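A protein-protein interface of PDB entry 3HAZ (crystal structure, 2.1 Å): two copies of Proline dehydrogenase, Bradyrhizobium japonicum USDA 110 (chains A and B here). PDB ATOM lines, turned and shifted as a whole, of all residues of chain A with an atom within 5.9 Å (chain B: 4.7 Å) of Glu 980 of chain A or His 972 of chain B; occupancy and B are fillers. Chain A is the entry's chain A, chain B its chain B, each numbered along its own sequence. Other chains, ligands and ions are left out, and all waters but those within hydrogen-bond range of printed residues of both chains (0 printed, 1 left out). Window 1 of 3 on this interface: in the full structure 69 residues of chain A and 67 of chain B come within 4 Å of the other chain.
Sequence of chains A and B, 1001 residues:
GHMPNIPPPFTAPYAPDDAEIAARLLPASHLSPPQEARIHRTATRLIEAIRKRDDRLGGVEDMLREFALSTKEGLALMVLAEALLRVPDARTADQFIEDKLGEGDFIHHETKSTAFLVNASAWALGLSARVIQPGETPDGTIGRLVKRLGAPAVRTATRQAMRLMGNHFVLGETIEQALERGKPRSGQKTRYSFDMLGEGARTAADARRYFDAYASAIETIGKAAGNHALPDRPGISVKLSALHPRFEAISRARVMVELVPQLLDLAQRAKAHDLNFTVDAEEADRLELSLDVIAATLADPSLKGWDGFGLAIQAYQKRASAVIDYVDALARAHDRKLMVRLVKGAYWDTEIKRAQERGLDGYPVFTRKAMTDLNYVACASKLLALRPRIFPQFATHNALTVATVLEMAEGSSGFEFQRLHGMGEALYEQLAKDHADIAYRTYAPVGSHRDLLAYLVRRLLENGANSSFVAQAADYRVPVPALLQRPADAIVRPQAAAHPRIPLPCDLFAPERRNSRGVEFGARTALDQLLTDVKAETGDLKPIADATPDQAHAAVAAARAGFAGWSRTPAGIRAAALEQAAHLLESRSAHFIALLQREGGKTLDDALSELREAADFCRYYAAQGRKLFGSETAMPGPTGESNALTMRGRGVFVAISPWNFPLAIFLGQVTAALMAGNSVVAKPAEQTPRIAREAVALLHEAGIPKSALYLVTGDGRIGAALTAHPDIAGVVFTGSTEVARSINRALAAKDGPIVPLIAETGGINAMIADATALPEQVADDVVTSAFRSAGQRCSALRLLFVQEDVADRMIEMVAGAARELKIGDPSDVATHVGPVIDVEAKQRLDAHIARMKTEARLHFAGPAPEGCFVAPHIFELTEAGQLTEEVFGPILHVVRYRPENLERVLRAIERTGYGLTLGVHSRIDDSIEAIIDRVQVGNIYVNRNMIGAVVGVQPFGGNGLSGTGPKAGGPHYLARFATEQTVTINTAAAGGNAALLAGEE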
ATOM      1  N   LEU A 628     -14.340 -11.614  23.566  1.00  0.00           N
ATOM      2  CA  LEU A 628     -13.086 -12.005  22.934  1.00  0.00           C
ATOM      3  C   LEU A 628     -12.056 -10.875  22.874  1.00  0.00           C
ATOM      4  O   LEU A 628     -10.876 -11.094  23.136  1.00  0.00           O
ATOM      5  CB  LEU A 628     -13.342 -12.548  21.527  1.00  0.00           C
ATOM      6  CG  LEU A 628     -12.151 -13.228  20.850  1.00  0.00           C
ATOM      7  CD1 LEU A 628     -11.457 -14.169  21.819  1.00  0.00           C
ATOM      8  CD2 LEU A 628     -12.591 -13.983  19.598  1.00  0.00           C
ATOM      9  N   LEU A 645      -2.032 -12.541  26.434  1.00  0.00           N
ATOM     10  CA  LEU A 645      -2.465 -12.891  25.083  1.00  0.00           C
ATOM     11  C   LEU A 645      -3.565 -11.940  24.609  1.00  0.00           C
ATOM     12  O   LEU A 645      -4.561 -11.716  25.310  1.00  0.00           O
ATOM     13  CB  LEU A 645      -2.973 -14.339  25.048  1.00  0.00           C
ATOM     14  CG  LEU A 645      -3.399 -14.944  23.705  1.00  0.00           C
ATOM     15  CD1 LEU A 645      -2.233 -15.006  22.718  1.00  0.00           C
ATOM     16  CD2 LEU A 645      -3.986 -16.338  23.912  1.00  0.00           C
ATOM     17  N   THR A 646      -3.378 -11.368  23.425  1.00  0.00           N
ATOM     18  CA  THR A 646      -4.376 -10.470  22.855  1.00  0.00           C
ATOM     19  C   THR A 646      -4.747 -10.922  21.447  1.00  0.00           C
ATOM     20  O   THR A 646      -4.064 -11.759  20.857  1.00  0.00           O
ATOM     21  CB  THR A 646      -3.880  -9.004  22.819  1.00  0.00           C
ATOM     22  OG1 THR A 646      -2.609  -8.945  22.172  1.00  0.00           O
ATOM     23  CG2 THR A 646      -3.727  -8.445  24.227  1.00  0.00           C
ATOM     24  N   MET A 647      -5.834 -10.366  20.924  1.00  0.00           N
ATOM     25  CA  MET A 647      -6.300 -10.661  19.575  1.00  0.00           C
ATOM     26  C   MET A 647      -6.484  -9.358  18.825  1.00  0.00           C
ATOM     27  O   MET A 647      -7.256  -8.496  19.239  1.00  0.00           O
ATOM     28  CB  MET A 647      -7.640 -11.380  19.624  1.00  0.00           C
ATOM     29  CG  MET A 647      -7.686 -12.509  20.614  1.00  0.00           C
ATOM     30  SD  MET A 647      -7.200 -14.037  19.829  1.00  0.00           S
ATOM     31  CE  MET A 647      -8.712 -14.379  18.941  1.00  0.00           C
ATOM     32  N   ARG A 648      -5.792  -9.220  17.708  1.00  0.00           N
ATOM     33  CA  ARG A 648      -5.821  -7.971  16.975  1.00  0.00           C
ATOM     34  C   ARG A 648      -6.416  -8.202  15.596  1.00  0.00           C
ATOM     35  O   ARG A 648      -6.381  -9.319  15.081  1.00  0.00           O
ATOM     36  CB  ARG A 648      -4.402  -7.404  16.870  1.00  0.00           C
ATOM     37  CG  ARG A 648      -3.665  -7.373  18.204  1.00  0.00           C
ATOM     38  CD  ARG A 648      -2.238  -6.838  18.074  1.00  0.00           C
ATOM     39  NE  ARG A 648      -2.183  -5.598  17.306  1.00  0.00           N
ATOM     40  CZ  ARG A 648      -1.294  -4.626  17.503  1.00  0.00           C
ATOM     41  NH1 ARG A 648      -1.334  -3.539  16.742  1.00  0.00           N
ATOM     42  NH2 ARG A 648      -0.376  -4.731  18.461  1.00  0.00           N
ATOM     43  N   ALA A 975     -12.828 -15.235  16.173  1.00  0.00           N
ATOM     44  CA  ALA A 975     -11.401 -15.479  16.347  1.00  0.00           C
ATOM     45  C   ALA A 975     -10.689 -15.645  15.011  1.00  0.00           C
ATOM     46  O   ALA A 975      -9.543 -15.230  14.858  1.00  0.00           O
ATOM     47  CB  ALA A 975     -11.170 -16.708  17.226  1.00  0.00           C
ATOM     48  N   ALA A 978      -9.223 -12.571  13.404  1.00  0.00           N
ATOM     49  CA  ALA A 978      -8.182 -11.867  14.147  1.00  0.00           C
ATOM     50  C   ALA A 978      -6.880 -12.652  14.190  1.00  0.00           C
ATOM     51  O   ALA A 978      -6.828 -13.808  13.778  1.00  0.00           O
ATOM     52  CB  ALA A 978      -8.657 -11.548  15.562  1.00  0.00           C
ATOM     53  N   THR A 979      -5.827 -12.007  14.687  1.00  0.00           N
ATOM     54  CA  THR A 979      -4.548 -12.665  14.862  1.00  0.00           C
ATOM     55  C   THR A 979      -4.122 -12.538  16.319  1.00  0.00           C
ATOM     56  O   THR A 979      -4.421 -11.535  16.971  1.00  0.00           O
ATOM     57  CB  THR A 979      -3.468 -12.061  13.914  1.00  0.00           C
ATOM     58  OG1 THR A 979      -2.281 -12.857  13.958  1.00  0.00           O
ATOM     59  CG2 THR A 979      -3.129 -10.631  14.307  1.00  0.00           C
ATOM     60  N   GLU A 980      -3.436 -13.557  16.831  1.00  0.00           N
ATOM     61  CA  GLU A 980      -2.974 -13.551  18.219  1.00  0.00           C
ATOM     62  C   GLU A 980      -1.665 -12.785  18.410  1.00  0.00           C
ATOM     63  O   GLU A 980      -0.811 -12.765  17.527  1.00  0.00           O
ATOM     64  CB  GLU A 980      -2.749 -14.975  18.713  1.00  0.00           C
ATOM     65  CG  GLU A 980      -4.004 -15.789  19.003  1.00  0.00           C
ATOM     66  CD  GLU A 980      -3.707 -17.270  18.978  1.00  0.00           C
ATOM     67  OE1 GLU A 980      -3.538 -17.870  20.063  1.00  0.00           O
ATOM     68  OE2 GLU A 980      -3.601 -17.826  17.866  1.00  0.00           O
ATOM     69  N   GLN A 981      -1.499 -12.198  19.589  1.00  0.00           N
ATOM     70  CA  GLN A 981      -0.237 -11.574  19.968  1.00  0.00           C
ATOM     71  C   GLN A 981       0.043 -11.808  21.444  1.00  0.00           C
ATOM     72  O   GLN A 981      -0.779 -11.485  22.301  1.00  0.00           O
ATOM     73  CB  GLN A 981      -0.247 -10.075  19.672  1.00  0.00           C
ATOM     74  CG  GLN A 981       1.074  -9.381  19.994  1.00  0.00           C
ATOM     75  CD  GLN A 981       1.138  -7.975  19.438  1.00  0.00           C
ATOM     76  OE1 GLN A 981       0.508  -7.061  19.969  1.00  0.00           O
ATOM     77  NE2 GLN A 981       1.905  -7.794  18.363  1.00  0.00           N
ATOM     78  N   THR A 982       1.206 -12.379  21.731  1.00  0.00           N
ATOM     79  CA  THR A 982       1.645 -12.586  23.103  1.00  0.00           C
ATOM     80  C   THR A 982       2.668 -11.523  23.484  1.00  0.00           C
ATOM     81  O   THR A 982       3.654 -11.315  22.774  1.00  0.00           O
ATOM     82  CB  THR A 982       2.290 -13.969  23.266  1.00  0.00           C
ATOM     83  OG1 THR A 982       1.365 -14.979  22.846  1.00  0.00           O
ATOM     84  CG2 THR A 982       2.713 -14.208  24.718  1.00  0.00           C
ATOM     85  N   GLY B 938       4.046 -11.756  16.331  1.00  0.00           N
ATOM     86  CA  GLY B 938       3.382 -12.779  17.124  1.00  0.00           C
ATOM     87  C   GLY B 938       3.773 -12.813  18.594  1.00  0.00           C
ATOM     88  O   GLY B 938       2.917 -12.968  19.461  1.00  0.00           O
ATOM     89  N   ASN B 959       2.619 -14.019  12.400  1.00  0.00           N
ATOM     90  CA  ASN B 959       1.713 -13.721  11.307  1.00  0.00           C
ATOM     91  C   ASN B 959       2.492 -13.170  10.131  1.00  0.00           C
ATOM     92  O   ASN B 959       3.726 -13.202  10.134  1.00  0.00           O
ATOM     93  CB  ASN B 959       0.640 -12.732  11.758  1.00  0.00           C
ATOM     94  CG  ASN B 959       1.149 -11.766  12.801  1.00  0.00           C
ATOM     95  OD1 ASN B 959       0.648 -11.730  13.928  1.00  0.00           O
ATOM     96  ND2 ASN B 959       2.167 -10.992  12.442  1.00  0.00           N
ATOM     97  N   PRO B 966      -3.370 -20.871  14.113  1.00  0.00           N
ATOM     98  CA  PRO B 966      -3.318 -20.304  15.464  1.00  0.00           C
ATOM     99  C   PRO B 966      -2.004 -20.672  16.149  1.00  0.00           C
ATOM    100  O   PRO B 966      -1.293 -21.563  15.673  1.00  0.00           O
ATOM    101  CB  PRO B 966      -4.493 -20.992  16.171  1.00  0.00           C
ATOM    102  CG  PRO B 966      -4.655 -22.287  15.458  1.00  0.00           C
ATOM    103  CD  PRO B 966      -4.226 -22.072  14.041  1.00  0.00           C
ATOM    104  N   LYS B 967      -1.694 -19.990  17.248  1.00  0.00           N
ATOM    105  CA  LYS B 967      -0.443 -20.204  17.972  1.00  0.00           C
ATOM    106  C   LYS B 967      -0.392 -21.566  18.653  1.00  0.00           C
ATOM    107  O   LYS B 967      -1.294 -21.927  19.408  1.00  0.00           O
ATOM    108  CB  LYS B 967      -0.267 -19.139  19.057  1.00  0.00           C
ATOM    109  CG  LYS B 967       0.026 -17.725  18.581  1.00  0.00           C
ATOM    110  CD  LYS B 967      -0.163 -16.762  19.765  1.00  0.00           C
ATOM    111  CE  LYS B 967       0.532 -15.417  19.562  1.00  0.00           C
ATOM    112  NZ  LYS B 967       2.006 -15.548  19.627  1.00  0.00           N
ATOM    113  N   GLY B 970      -1.122 -22.621  22.739  1.00  0.00           N
ATOM    114  CA  GLY B 970      -2.061 -21.607  23.189  1.00  0.00           C
ATOM    115  C   GLY B 970      -3.493 -22.108  23.095  1.00  0.00           C
ATOM    116  O   GLY B 970      -3.743 -23.172  22.526  1.00  0.00           O
ATOM    117  N   PRO B 971      -4.447 -21.333  23.627  1.00  0.00           N
ATOM    118  CA  PRO B 971      -5.829 -21.800  23.767  1.00  0.00           C
ATOM    119  C   PRO B 971      -6.629 -21.792  22.468  1.00  0.00           C
ATOM    120  O   PRO B 971      -7.791 -22.171  22.511  1.00  0.00           O
ATOM    121  CB  PRO B 971      -6.455 -20.793  24.754  1.00  0.00           C
ATOM    122  CG  PRO B 971      -5.386 -19.762  25.051  1.00  0.00           C
ATOM    123  CD  PRO B 971      -4.295 -19.932  24.043  1.00  0.00           C
ATOM    124  N   HIS B 972      -6.048 -21.370  21.349  1.00  0.00           N
ATOM    125  CA  HIS B 972      -6.796 -21.372  20.091  1.00  0.00           C
ATOM    126  C   HIS B 972      -6.312 -22.438  19.116  1.00  0.00           C
ATOM    127  O   HIS B 972      -6.797 -22.518  17.991  1.00  0.00           O
ATOM    128  CB  HIS B 972      -6.739 -20.004  19.409  1.00  0.00           C
ATOM    129  CG  HIS B 972      -7.255 -18.888  20.260  1.00  0.00           C
ATOM    130  ND1 HIS B 972      -8.600 -18.670  20.466  1.00  0.00           N
ATOM    131  CD2 HIS B 972      -6.606 -17.925  20.957  1.00  0.00           C
ATOM    132  CE1 HIS B 972      -8.757 -17.624  21.257  1.00  0.00           C
ATOM    133  NE2 HIS B 972      -7.562 -17.154  21.570  1.00  0.00           N
ATOM    134  N   TYR B 973      -5.367 -23.260  19.554  1.00  0.00           N
ATOM    135  CA  TYR B 973      -4.704 -24.208  18.658  1.00  0.00           C
ATOM    136  C   TYR B 973      -5.565 -25.416  18.287  1.00  0.00           C
ATOM    137  O   TYR B 973      -5.730 -25.730  17.110  1.00  0.00           O
ATOM    138  CB  TYR B 973      -3.411 -24.691  19.305  1.00  0.00           C
ATOM    139  CG  TYR B 973      -2.408 -25.311  18.360  1.00  0.00           C
ATOM    140  CD1 TYR B 973      -1.834 -24.565  17.337  1.00  0.00           C
ATOM    141  CD2 TYR B 973      -1.992 -26.629  18.524  1.00  0.00           C
ATOM    142  CE1 TYR B 973      -0.891 -25.121  16.482  1.00  0.00           C
ATOM    143  CE2 TYR B 973      -1.050 -27.191  17.684  1.00  0.00           C
ATOM    144  CZ  TYR B 973      -0.505 -26.429  16.665  1.00  0.00           C
ATOM    145  OH  TYR B 973       0.427 -26.982  15.831  1.00  0.00           O
ATOM    146  N   LEU B 974      -6.099 -26.095  19.296  1.00  0.00           N
ATOM    147  CA  LEU B 974      -6.811 -27.356  19.082  1.00  0.00           C
ATOM    148  C   LEU B 974      -8.038 -27.224  18.185  1.00  0.00           C
ATOM    149  O   LEU B 974      -8.266 -28.061  17.312  1.00  0.00           O
ATOM    150  CB  LEU B 974      -7.202 -27.981  20.418  1.00  0.00           C
ATOM    151  CG  LEU B 974      -6.000 -28.481  21.223  1.00  0.00           C
ATOM    152  CD1 LEU B 974      -6.447 -29.250  22.459  1.00  0.00           C
ATOM    153  CD2 LEU B 974      -5.087 -29.342  20.353  1.00  0.00           C
ATOM    154  N   ALA B 975      -8.822 -26.174  18.411  1.00  0.00           N
ATOM    155  CA  ALA B 975     -10.033 -25.913  17.635  1.00  0.00           C
ATOM    156  C   ALA B 975      -9.819 -26.017  16.130  1.00  0.00           C
ATOM    157  O   ALA B 975     -10.682 -26.513  15.401  1.00  0.00           O
ATOM    158  CB  ALA B 975     -10.595 -24.541  17.984  1.00  0.00           C
ATOM    159  N   ARG B 976      -8.675 -25.529  15.660  1.00  0.00           N
ATOM    160  CA  ARG B 976      -8.408 -25.494  14.228  1.00  0.00           C
ATOM    161  C   ARG B 976      -8.310 -26.893  13.632  1.00  0.00           C
ATOM    162  O   ARG B 976      -8.520 -27.069  12.436  1.00  0.00           O
ATOM    163  CB  ARG B 976      -7.138 -24.696  13.933  1.00  0.00           C
ATOM    164  CG  ARG B 976      -6.901 -24.444  12.466  1.00  0.00           C
ATOM    165  CD  ARG B 976      -7.725 -23.276  11.944  1.00  0.00           C
ATOM    166  NE  ARG B 976      -7.226 -22.868  10.633  1.00  0.00           N
ATOM    167  CZ  ARG B 976      -7.834 -23.128   9.479  1.00  0.00           C
ATOM    168  NH1 ARG B 976      -7.288 -22.726   8.338  1.00  0.00           N
ATOM    169  NH2 ARG B 976      -8.992 -23.779   9.460  1.00  0.00           N
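The side-chain sulfur (SD) of Met 647 of chain A is in hydrogen-bond range of a ring nitrogen (NE2) of His 972 of chain B.
OG1 of Thr 979 of chain A lies within hydrogen-bond range of OD1 of Asn 959 of chain B, at 3.1 Å.
OE2 of Glu 980 of chain A sits at hydrogen-bond distance from N of Lys 967 of chain B.
O of Gly 938 of chain B sits at hydrogen-bond distance from N of Thr 982 of chain A, 2.9 Å away.
The side-chain amino group of Lys 967 of chain B lies within hydrogen-bond range of the side-chain hydroxyl of Thr 982 of chain A (3.3 Å).
The backbone NH (N) of Thr 646 of chain A sits at hydrogen-bond distance from the backbone carbonyl oxygen (O) of Gln 981 of chain A (2.8 Å).
O of Arg 648 of chain A sits at hydrogen-bond distance from N of Thr 979 of chain A.
NH2 of Arg 648 of chain A is in hydrogen-bond range of OE1 of Gln 981 of chain A (2.9 Å).
The side-chain amino group (NZ) of Lys 967 of chain B is in hydrogen-bond range of the backbone carbonyl oxygen (O) of Gly 938 of chain B, at 2.7 Å.
Among the printed residues, merely in contact across the chains: Leu 645 of chain A with Pro 971 of chain B, Glu 980 of chain A with Pro 966 of chain B, Glu 980 of chain A with His 972 of chain B, Gln 981 of chain A with Gly 938 of chain B and Gln 981 of chain A with Lys 967 of chain B.
Of the printed residues of chain B, Glu 980 of chain A touches Pro 966, Lys 967 and His 972.
His 972 of chain B touches just these residues of chain A: Met 647 and Glu 980.
Of the printed residues of chain B, Gln 981 of chain A touches Gly 938 and Lys 967.
Of the printed residues of chain A, Asn 959 of chain B touches Thr 979 (3.1 Å).
Arg 976 of chain B touches none of the printed residues of chain A.
Thr 646 of chain A touches none of the printed residues of chain B.
The nearest printed residue of chain B that does not touch Glu 980 of chain A is Asn 959 of chain B (4.02 Å).
The nearest residue of chain A that does not touch His 972 of chain B is Leu 645 of chain A (4.3 Å).
Hydrophobic or aromatic side chains of chain A that line the printed part of chain B: Leu 645 and Met 647.
Hydrophobic or aromatic side chains of chain B within 4 Å of the printed part of chain A: Pro 966, Pro 971 and His 972.
Among the printed residues, no Asp or Glu carboxylate lies within 4 Å of a Lys or Arg side-chain nitrogen of the other chain.
1 position is printed for both chains.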
